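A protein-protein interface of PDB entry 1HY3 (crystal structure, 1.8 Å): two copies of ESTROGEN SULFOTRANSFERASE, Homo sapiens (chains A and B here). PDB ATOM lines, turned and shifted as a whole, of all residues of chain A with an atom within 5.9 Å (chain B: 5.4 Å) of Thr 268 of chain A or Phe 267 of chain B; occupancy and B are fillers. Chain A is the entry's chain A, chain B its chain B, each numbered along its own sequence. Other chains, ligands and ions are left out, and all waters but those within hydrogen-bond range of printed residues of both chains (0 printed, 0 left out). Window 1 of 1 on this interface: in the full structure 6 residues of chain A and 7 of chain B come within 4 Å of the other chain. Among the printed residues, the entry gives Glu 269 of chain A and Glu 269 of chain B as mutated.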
ATOM      1  N   PRO A 155      16.764   0.249 -32.762  1.00  0.00           N
ATOM      2  CA  PRO A 155      16.221  -0.799 -31.893  1.00  0.00           C
ATOM      3  C   PRO A 155      14.722  -1.011 -32.117  1.00  0.00           C
ATOM      4  O   PRO A 155      14.232  -2.138 -32.085  1.00  0.00           O
ATOM      5  CB  PRO A 155      16.535  -0.283 -30.490  1.00  0.00           C
ATOM      6  CG  PRO A 155      17.793   0.541 -30.699  1.00  0.00           C
ATOM      7  CD  PRO A 155      17.474   1.279 -31.976  1.00  0.00           C
ATOM      8  N   HIS A 266      25.939  -1.221 -35.583  1.00  0.00           N
ATOM      9  CA  HIS A 266      24.594  -0.735 -35.305  1.00  0.00           C
ATOM     10  C   HIS A 266      23.904  -1.347 -34.087  1.00  0.00           C
ATOM     11  O   HIS A 266      23.233  -0.634 -33.344  1.00  0.00           O
ATOM     12  CB  HIS A 266      23.716  -0.903 -36.549  1.00  0.00           C
ATOM     13  CG  HIS A 266      24.155  -0.057 -37.704  1.00  0.00           C
ATOM     14  ND1 HIS A 266      25.137  -0.454 -38.587  1.00  0.00           N
ATOM     15  CD2 HIS A 266      23.793   1.191 -38.085  1.00  0.00           C
ATOM     16  CE1 HIS A 266      25.360   0.511 -39.460  1.00  0.00           C
ATOM     17  NE2 HIS A 266      24.558   1.521 -39.178  1.00  0.00           N
ATOM     18  N   PHE A 267      24.066  -2.649 -33.879  1.00  0.00           N
ATOM     19  CA  PHE A 267      23.455  -3.306 -32.726  1.00  0.00           C
ATOM     20  C   PHE A 267      24.239  -3.010 -31.453  1.00  0.00           C
ATOM     21  O   PHE A 267      25.469  -3.069 -31.447  1.00  0.00           O
ATOM     22  CB  PHE A 267      23.436  -4.826 -32.893  1.00  0.00           C
ATOM     23  CG  PHE A 267      22.367  -5.339 -33.811  1.00  0.00           C
ATOM     24  CD1 PHE A 267      22.424  -5.097 -35.181  1.00  0.00           C
ATOM     25  CD2 PHE A 267      21.334  -6.128 -33.313  1.00  0.00           C
ATOM     26  CE1 PHE A 267      21.467  -5.648 -36.044  1.00  0.00           C
ATOM     27  CE2 PHE A 267      20.376  -6.680 -34.165  1.00  0.00           C
ATOM     28  CZ  PHE A 267      20.445  -6.439 -35.534  1.00  0.00           C
ATOM     29  N   THR A 268      23.519  -2.693 -30.381  1.00  0.00           N
ATOM     30  CA  THR A 268      24.141  -2.454 -29.086  1.00  0.00           C
ATOM     31  C   THR A 268      24.304  -3.860 -28.511  1.00  0.00           C
ATOM     32  O   THR A 268      23.755  -4.821 -29.055  1.00  0.00           O
ATOM     33  CB  THR A 268      23.217  -1.656 -28.158  1.00  0.00           C
ATOM     34  OG1 THR A 268      21.981  -2.368 -27.996  1.00  0.00           O
ATOM     35  CG2 THR A 268      22.928  -0.292 -28.737  1.00  0.00           C
ATOM     36  N   GLU A 269      25.046  -3.996 -27.421  1.00  0.00           N
ATOM     37  CA  GLU A 269      25.227  -5.314 -26.836  1.00  0.00           C
ATOM     38  C   GLU A 269      23.871  -5.885 -26.433  1.00  0.00           C
ATOM     39  O   GLU A 269      23.599  -7.063 -26.635  1.00  0.00           O
ATOM     40  CB  GLU A 269      26.140  -5.241 -25.609  1.00  0.00           C
ATOM     41  CG  GLU A 269      26.588  -6.608 -25.093  1.00  0.00           C
ATOM     42  CD  GLU A 269      25.500  -7.352 -24.337  1.00  0.00           C
ATOM     43  OE1 GLU A 269      25.591  -8.596 -24.237  1.00  0.00           O
ATOM     44  OE2 GLU A 269      24.560  -6.695 -23.831  1.00  0.00           O
ATOM     45  N   ALA A 270      23.021  -5.037 -25.867  1.00  0.00           N
ATOM     46  CA  ALA A 270      21.703  -5.465 -25.410  1.00  0.00           C
ATOM     47  C   ALA A 270      20.792  -5.899 -26.552  1.00  0.00           C
ATOM     48  O   ALA A 270      20.067  -6.893 -26.432  1.00  0.00           O
ATOM     49  CB  ALA A 270      21.047  -4.348 -24.619  1.00  0.00           C
ATOM     50  N   LEU A 271      20.818  -5.154 -27.654  1.00  0.00           N
ATOM     51  CA  LEU A 271      19.968  -5.490 -28.794  1.00  0.00           C
ATOM     52  C   LEU A 271      20.455  -6.769 -29.448  1.00  0.00           C
ATOM     53  O   LEU A 271      19.655  -7.607 -29.876  1.00  0.00           O
ATOM     54  CB  LEU A 271      19.954  -4.352 -29.818  1.00  0.00           C
ATOM     55  CG  LEU A 271      18.987  -4.565 -30.989  1.00  0.00           C
ATOM     56  CD1 LEU A 271      17.569  -4.678 -30.457  1.00  0.00           C
ATOM     57  CD2 LEU A 271      19.088  -3.398 -31.964  1.00  0.00           C
ATOM     58  N   ASN A 272      21.773  -6.929 -29.507  1.00  0.00           N
ATOM     59  CA  ASN A 272      22.364  -8.120 -30.101  1.00  0.00           C
ATOM     60  C   ASN A 272      21.984  -9.355 -29.286  1.00  0.00           C
ATOM     61  O   ASN A 272      21.673 -10.410 -29.836  1.00  0.00           O
ATOM     62  CB  ASN A 272      23.889  -7.985 -30.151  1.00  0.00           C
ATOM     63  CG  ASN A 272      24.534  -9.028 -31.039  1.00  0.00           C
ATOM     64  OD1 ASN A 272      24.164  -9.175 -32.206  1.00  0.00           O
ATOM     65  ND2 ASN A 272      25.503  -9.755 -30.498  1.00  0.00           N
ATOM     66  N   GLU A 273      21.998  -9.211 -27.966  1.00  0.00           N
ATOM     67  CA  GLU A 273      21.662 -10.325 -27.092  1.00  0.00           C
ATOM     68  C   GLU A 273      20.210 -10.757 -27.298  1.00  0.00           C
ATOM     69  O   GLU A 273      19.914 -11.944 -27.432  1.00  0.00           O
ATOM     70  CB  GLU A 273      21.893  -9.916 -25.636  1.00  0.00           C
ATOM     71  CG  GLU A 273      21.889 -11.070 -24.666  1.00  0.00           C
ATOM     72  CD  GLU A 273      22.142 -10.612 -23.242  1.00  0.00           C
ATOM     73  OE1 GLU A 273      23.110  -9.843 -23.024  1.00  0.00           O
ATOM     74  OE2 GLU A 273      21.375 -11.024 -22.348  1.00  0.00           O
ATOM     75  N   LYS B 132      32.801   1.839 -18.681  1.00  0.00           N
ATOM     76  CA  LYS B 132      31.743   1.977 -19.680  1.00  0.00           C
ATOM     77  C   LYS B 132      30.500   2.692 -19.156  1.00  0.00           C
ATOM     78  O   LYS B 132      29.929   3.518 -19.857  1.00  0.00           O
ATOM     79  CB  LYS B 132      31.358   0.611 -20.239  1.00  0.00           C
ATOM     80  CG  LYS B 132      32.434  -0.041 -21.098  1.00  0.00           C
ATOM     81  CD  LYS B 132      31.930  -1.405 -21.553  1.00  0.00           C
ATOM     82  CE  LYS B 132      33.024  -2.265 -22.126  1.00  0.00           C
ATOM     83  NZ  LYS B 132      32.492  -3.610 -22.466  1.00  0.00           N
ATOM     84  N   ALA B 135      31.321   6.292 -18.726  1.00  0.00           N
ATOM     85  CA  ALA B 135      31.344   6.968 -20.016  1.00  0.00           C
ATOM     86  C   ALA B 135      29.937   7.372 -20.459  1.00  0.00           C
ATOM     87  O   ALA B 135      29.733   8.477 -20.972  1.00  0.00           O
ATOM     88  CB  ALA B 135      31.999   6.070 -21.071  1.00  0.00           C
ATOM     89  N   VAL B 136      28.973   6.479 -20.259  1.00  0.00           N
ATOM     90  CA  VAL B 136      27.592   6.771 -20.624  1.00  0.00           C
ATOM     91  C   VAL B 136      27.050   7.919 -19.784  1.00  0.00           C
ATOM     92  O   VAL B 136      26.484   8.877 -20.308  1.00  0.00           O
ATOM     93  CB  VAL B 136      26.684   5.540 -20.410  1.00  0.00           C
ATOM     94  CG1 VAL B 136      25.225   5.911 -20.658  1.00  0.00           C
ATOM     95  CG2 VAL B 136      27.107   4.415 -21.353  1.00  0.00           C
ATOM     96  N   PHE B 154      27.983   9.543 -29.616  1.00  0.00           N
ATOM     97  CA  PHE B 154      28.485   8.735 -28.511  1.00  0.00           C
ATOM     98  C   PHE B 154      29.839   8.118 -28.841  1.00  0.00           C
ATOM     99  O   PHE B 154      30.744   8.143 -28.010  1.00  0.00           O
ATOM    100  CB  PHE B 154      27.494   7.634 -28.133  1.00  0.00           C
ATOM    101  CG  PHE B 154      27.884   6.882 -26.893  1.00  0.00           C
ATOM    102  CD1 PHE B 154      28.187   5.528 -26.948  1.00  0.00           C
ATOM    103  CD2 PHE B 154      27.977   7.539 -25.668  1.00  0.00           C
ATOM    104  CE1 PHE B 154      28.580   4.838 -25.802  1.00  0.00           C
ATOM    105  CE2 PHE B 154      28.370   6.853 -24.513  1.00  0.00           C
ATOM    106  CZ  PHE B 154      28.669   5.506 -24.583  1.00  0.00           C
ATOM    107  N   VAL B 158      33.229   8.624 -26.696  1.00  0.00           N
ATOM    108  CA  VAL B 158      33.960   7.498 -26.132  1.00  0.00           C
ATOM    109  C   VAL B 158      35.425   7.581 -26.545  1.00  0.00           C
ATOM    110  O   VAL B 158      36.312   7.174 -25.800  1.00  0.00           O
ATOM    111  CB  VAL B 158      33.349   6.156 -26.596  1.00  0.00           C
ATOM    112  CG1 VAL B 158      34.244   5.005 -26.200  1.00  0.00           C
ATOM    113  CG2 VAL B 158      31.965   5.984 -25.967  1.00  0.00           C
ATOM    114  N   TRP B 263      25.744   0.545 -20.128  1.00  0.00           N
ATOM    115  CA  TRP B 263      26.617   0.587 -21.299  1.00  0.00           C
ATOM    116  C   TRP B 263      26.112  -0.375 -22.376  1.00  0.00           C
ATOM    117  O   TRP B 263      26.318  -0.150 -23.570  1.00  0.00           O
ATOM    118  CB  TRP B 263      28.060   0.227 -20.932  1.00  0.00           C
ATOM    119  CG  TRP B 263      28.257  -1.201 -20.458  1.00  0.00           C
ATOM    120  CD1 TRP B 263      28.284  -1.642 -19.164  1.00  0.00           C
ATOM    121  CD2 TRP B 263      28.503  -2.351 -21.278  1.00  0.00           C
ATOM    122  NE1 TRP B 263      28.538  -2.996 -19.127  1.00  0.00           N
ATOM    123  CE2 TRP B 263      28.677  -3.455 -20.413  1.00  0.00           C
ATOM    124  CE3 TRP B 263      28.594  -2.557 -22.667  1.00  0.00           C
ATOM    125  CZ2 TRP B 263      28.938  -4.752 -20.888  1.00  0.00           C
ATOM    126  CZ3 TRP B 263      28.852  -3.842 -23.136  1.00  0.00           C
ATOM    127  CH2 TRP B 263      29.020  -4.924 -22.245  1.00  0.00           C
ATOM    128  N   LYS B 264      25.449  -1.450 -21.955  1.00  0.00           N
ATOM    129  CA  LYS B 264      24.923  -2.434 -22.900  1.00  0.00           C
ATOM    130  C   LYS B 264      23.861  -1.831 -23.820  1.00  0.00           C
ATOM    131  O   LYS B 264      23.567  -2.370 -24.881  1.00  0.00           O
ATOM    132  CB  LYS B 264      24.327  -3.631 -22.143  1.00  0.00           C
ATOM    133  CG  LYS B 264      25.357  -4.443 -21.367  1.00  0.00           C
ATOM    134  CD  LYS B 264      24.706  -5.578 -20.589  1.00  0.00           C
ATOM    135  CE  LYS B 264      25.722  -6.331 -19.755  1.00  0.00           C
ATOM    136  NZ  LYS B 264      25.060  -7.367 -18.904  1.00  0.00           N
ATOM    137  N   ASN B 265      23.287  -0.708 -23.407  1.00  0.00           N
ATOM    138  CA  ASN B 265      22.255  -0.048 -24.190  1.00  0.00           C
ATOM    139  C   ASN B 265      22.814   1.053 -25.085  1.00  0.00           C
ATOM    140  O   ASN B 265      22.085   1.621 -25.905  1.00  0.00           O
ATOM    141  CB  ASN B 265      21.195   0.550 -23.253  1.00  0.00           C
ATOM    142  CG  ASN B 265      20.479  -0.505 -22.438  1.00  0.00           C
ATOM    143  OD1 ASN B 265      19.894  -1.431 -22.992  1.00  0.00           O
ATOM    144  ND2 ASN B 265      20.522  -0.373 -21.119  1.00  0.00           N
ATOM    145  N   HIS B 266      24.104   1.356 -24.934  1.00  0.00           N
ATOM    146  CA  HIS B 266      24.716   2.421 -25.724  1.00  0.00           C
ATOM    147  C   HIS B 266      25.866   2.034 -26.654  1.00  0.00           C
ATOM    148  O   HIS B 266      25.949   2.537 -27.775  1.00  0.00           O
ATOM    149  CB  HIS B 266      25.175   3.547 -24.796  1.00  0.00           C
ATOM    150  CG  HIS B 266      24.054   4.217 -24.067  1.00  0.00           C
ATOM    151  ND1 HIS B 266      23.515   3.712 -22.903  1.00  0.00           N
ATOM    152  CD2 HIS B 266      23.343   5.333 -24.358  1.00  0.00           C
ATOM    153  CE1 HIS B 266      22.520   4.488 -22.509  1.00  0.00           C
ATOM    154  NE2 HIS B 266      22.396   5.478 -23.375  1.00  0.00           N
ATOM    155  N   PHE B 267      26.752   1.159 -26.198  1.00  0.00           N
ATOM    156  CA  PHE B 267      27.891   0.728 -27.009  1.00  0.00           C
ATOM    157  C   PHE B 267      27.503  -0.255 -28.103  1.00  0.00           C
ATOM    158  O   PHE B 267      26.854  -1.254 -27.824  1.00  0.00           O
ATOM    159  CB  PHE B 267      28.951   0.026 -26.146  1.00  0.00           C
ATOM    160  CG  PHE B 267      29.785   0.951 -25.309  1.00  0.00           C
ATOM    161  CD1 PHE B 267      29.229   1.630 -24.226  1.00  0.00           C
ATOM    162  CD2 PHE B 267      31.137   1.123 -25.589  1.00  0.00           C
ATOM    163  CE1 PHE B 267      30.011   2.464 -23.431  1.00  0.00           C
ATOM    164  CE2 PHE B 267      31.929   1.953 -24.804  1.00  0.00           C
ATOM    165  CZ  PHE B 267      31.366   2.626 -23.719  1.00  0.00           C
ATOM    166  N   THR B 268      27.904   0.019 -29.343  1.00  0.00           N
ATOM    167  CA  THR B 268      27.641  -0.922 -30.425  1.00  0.00           C
ATOM    168  C   THR B 268      28.648  -2.034 -30.155  1.00  0.00           C
ATOM    169  O   THR B 268      29.594  -1.832 -29.394  1.00  0.00           O
ATOM    170  CB  THR B 268      27.955  -0.328 -31.817  1.00  0.00           C
ATOM    171  OG1 THR B 268      29.335   0.061 -31.872  1.00  0.00           O
ATOM    172  CG2 THR B 268      27.089   0.886 -32.092  1.00  0.00           C
ATOM    173  N   GLU B 269      28.458  -3.198 -30.768  1.00  0.00           N
ATOM    174  CA  GLU B 269      29.384  -4.306 -30.571  1.00  0.00           C
ATOM    175  C   GLU B 269      30.784  -3.904 -31.032  1.00  0.00           C
ATOM    176  O   GLU B 269      31.785  -4.325 -30.454  1.00  0.00           O
ATOM    177  CB  GLU B 269      28.920  -5.531 -31.342  1.00  0.00           C
ATOM    178  N   LEU B 271      32.139  -0.769 -31.049  1.00  0.00           N
ATOM    179  CA  LEU B 271      32.743   0.159 -30.099  1.00  0.00           C
ATOM    180  C   LEU B 271      33.117  -0.592 -28.832  1.00  0.00           C
ATOM    181  O   LEU B 271      34.118  -0.285 -28.185  1.00  0.00           O
ATOM    182  CB  LEU B 271      31.780   1.300 -29.760  1.00  0.00           C
ATOM    183  CG  LEU B 271      32.394   2.431 -28.922  1.00  0.00           C
ATOM    184  CD1 LEU B 271      33.503   3.104 -29.721  1.00  0.00           C
ATOM    185  CD2 LEU B 271      31.330   3.447 -28.554  1.00  0.00           C
ATOM    186  N   ASN B 272      32.311  -1.582 -28.469  1.00  0.00           N
ATOM    187  CA  ASN B 272      32.591  -2.355 -27.270  1.00  0.00           C
ATOM    188  C   ASN B 272      33.910  -3.093 -27.455  1.00  0.00           C
ATOM    189  O   ASN B 272      34.752  -3.132 -26.558  1.00  0.00           O
ATOM    190  CB  ASN B 272      31.469  -3.360 -27.008  1.00  0.00           C
ATOM    191  CG  ASN B 272      31.435  -3.817 -25.566  1.00  0.00           C
ATOM    192  OD1 ASN B 272      31.276  -3.001 -24.655  1.00  0.00           O
ATOM    193  ND2 ASN B 272      31.586  -5.121 -25.346  1.00  0.00           N
ATOM    194  N   PHE B 275      36.776  -0.527 -27.362  1.00  0.00           N
ATOM    195  CA  PHE B 275      36.963  -0.075 -25.987  1.00  0.00           C
ATOM    196  C   PHE B 275      37.595  -1.145 -25.096  1.00  0.00           C
ATOM    197  O   PHE B 275      38.504  -0.852 -24.307  1.00  0.00           O
ATOM    198  CB  PHE B 275      35.611   0.358 -25.407  1.00  0.00           C
ATOM    199  CG  PHE B 275      35.707   1.014 -24.059  1.00  0.00           C
ATOM    200  CD1 PHE B 275      35.835   0.247 -22.899  1.00  0.00           C
ATOM    201  CD2 PHE B 275      35.672   2.395 -23.949  1.00  0.00           C
ATOM    202  CE1 PHE B 275      35.926   0.857 -21.650  1.00  0.00           C
ATOM    203  CE2 PHE B 275      35.758   3.014 -22.710  1.00  0.00           C
ATOM    204  CZ  PHE B 275      35.886   2.244 -21.555  1.00  0.00           C
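OG1 of Thr 268 of chain A lies close to O of Lys 264 of chain B (3.5 Å).
N of Glu 269 of chain A sits at hydrogen-bond distance from O of Phe 267 of chain B, 3.3 Å away.
The backbone carbonyl oxygen (O) of Phe 267 of chain A lies within hydrogen-bond range of the backbone NH (N) of Glu 269 of chain B, 3.1 Å away.
O of Lys 264 of chain B sits at hydrogen-bond distance from N of Glu 269 of chain A, 3.4 Å away.
O of Lys 264 of chain B is in hydrogen-bond range of N of Ala 270 of chain A (2.9 Å).
The backbone NH (N) of Leu 271 of chain B is in hydrogen-bond range of the side-chain hydroxyl (OG1) of Thr 268 of chain B (3.0 Å).
The backbone NH (N) of Leu 271 of chain A lies within hydrogen-bond range of the side-chain hydroxyl (OG1) of Thr 268 of chain A.
Among the printed residues, merely in contact across the chains: Phe 267 of chain A with Thr 268 of chain B (3.2 Å), Thr 268 of chain A with Asn 265 of chain B (3.5 Å), Thr 268 of chain A with Phe 267 of chain B (3.2 Å), Glu 269 of chain A with Trp 263 of chain B (3.9 Å) and Ala 270 of chain A with Asn 265 of chain B (3.5 Å).
Of chain B, only Lys 264, Asn 265 and Phe 267 come within 4 Å of Thr 268 of chain A.
Of the printed residues of chain B, Ala 270 of chain A touches Lys 264 and Asn 265.
Of the printed residues of chain A, Trp 263 of chain B touches Glu 269 (3.9 Å).
His 266 of chain B touches none of the printed residues of chain A.
Phe 267 of chain B touches just these residues of chain A: Thr 268 and Glu 269.
Of the printed residues of chain A, Glu 269 of chain B touches Phe 267 (3.1 Å).
The nearest residue of chain B that does not touch Thr 268 of chain A is Thr 268 of chain B (4.05 Å).
The nearest printed residue of chain A that does not touch Asn 265 of chain B is Glu 269 of chain A (5.5 Å).
Of the 9 printed residues of chain A, 4 touch a printed residue of chain B.
Printed residues of chain A that touch a printed residue of chain B: Phe 267, Thr 268, Glu 269 and Ala 270.
Phe 267 of chain A touches Thr 268 of chain B, and with the chains exchanged Thr 268 of chain A touches Phe 267 of chain B.
Phe 267 of chain A touches Glu 269 of chain B, and with the chains exchanged Glu 269 of chain A touches Phe 267 of chain B.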
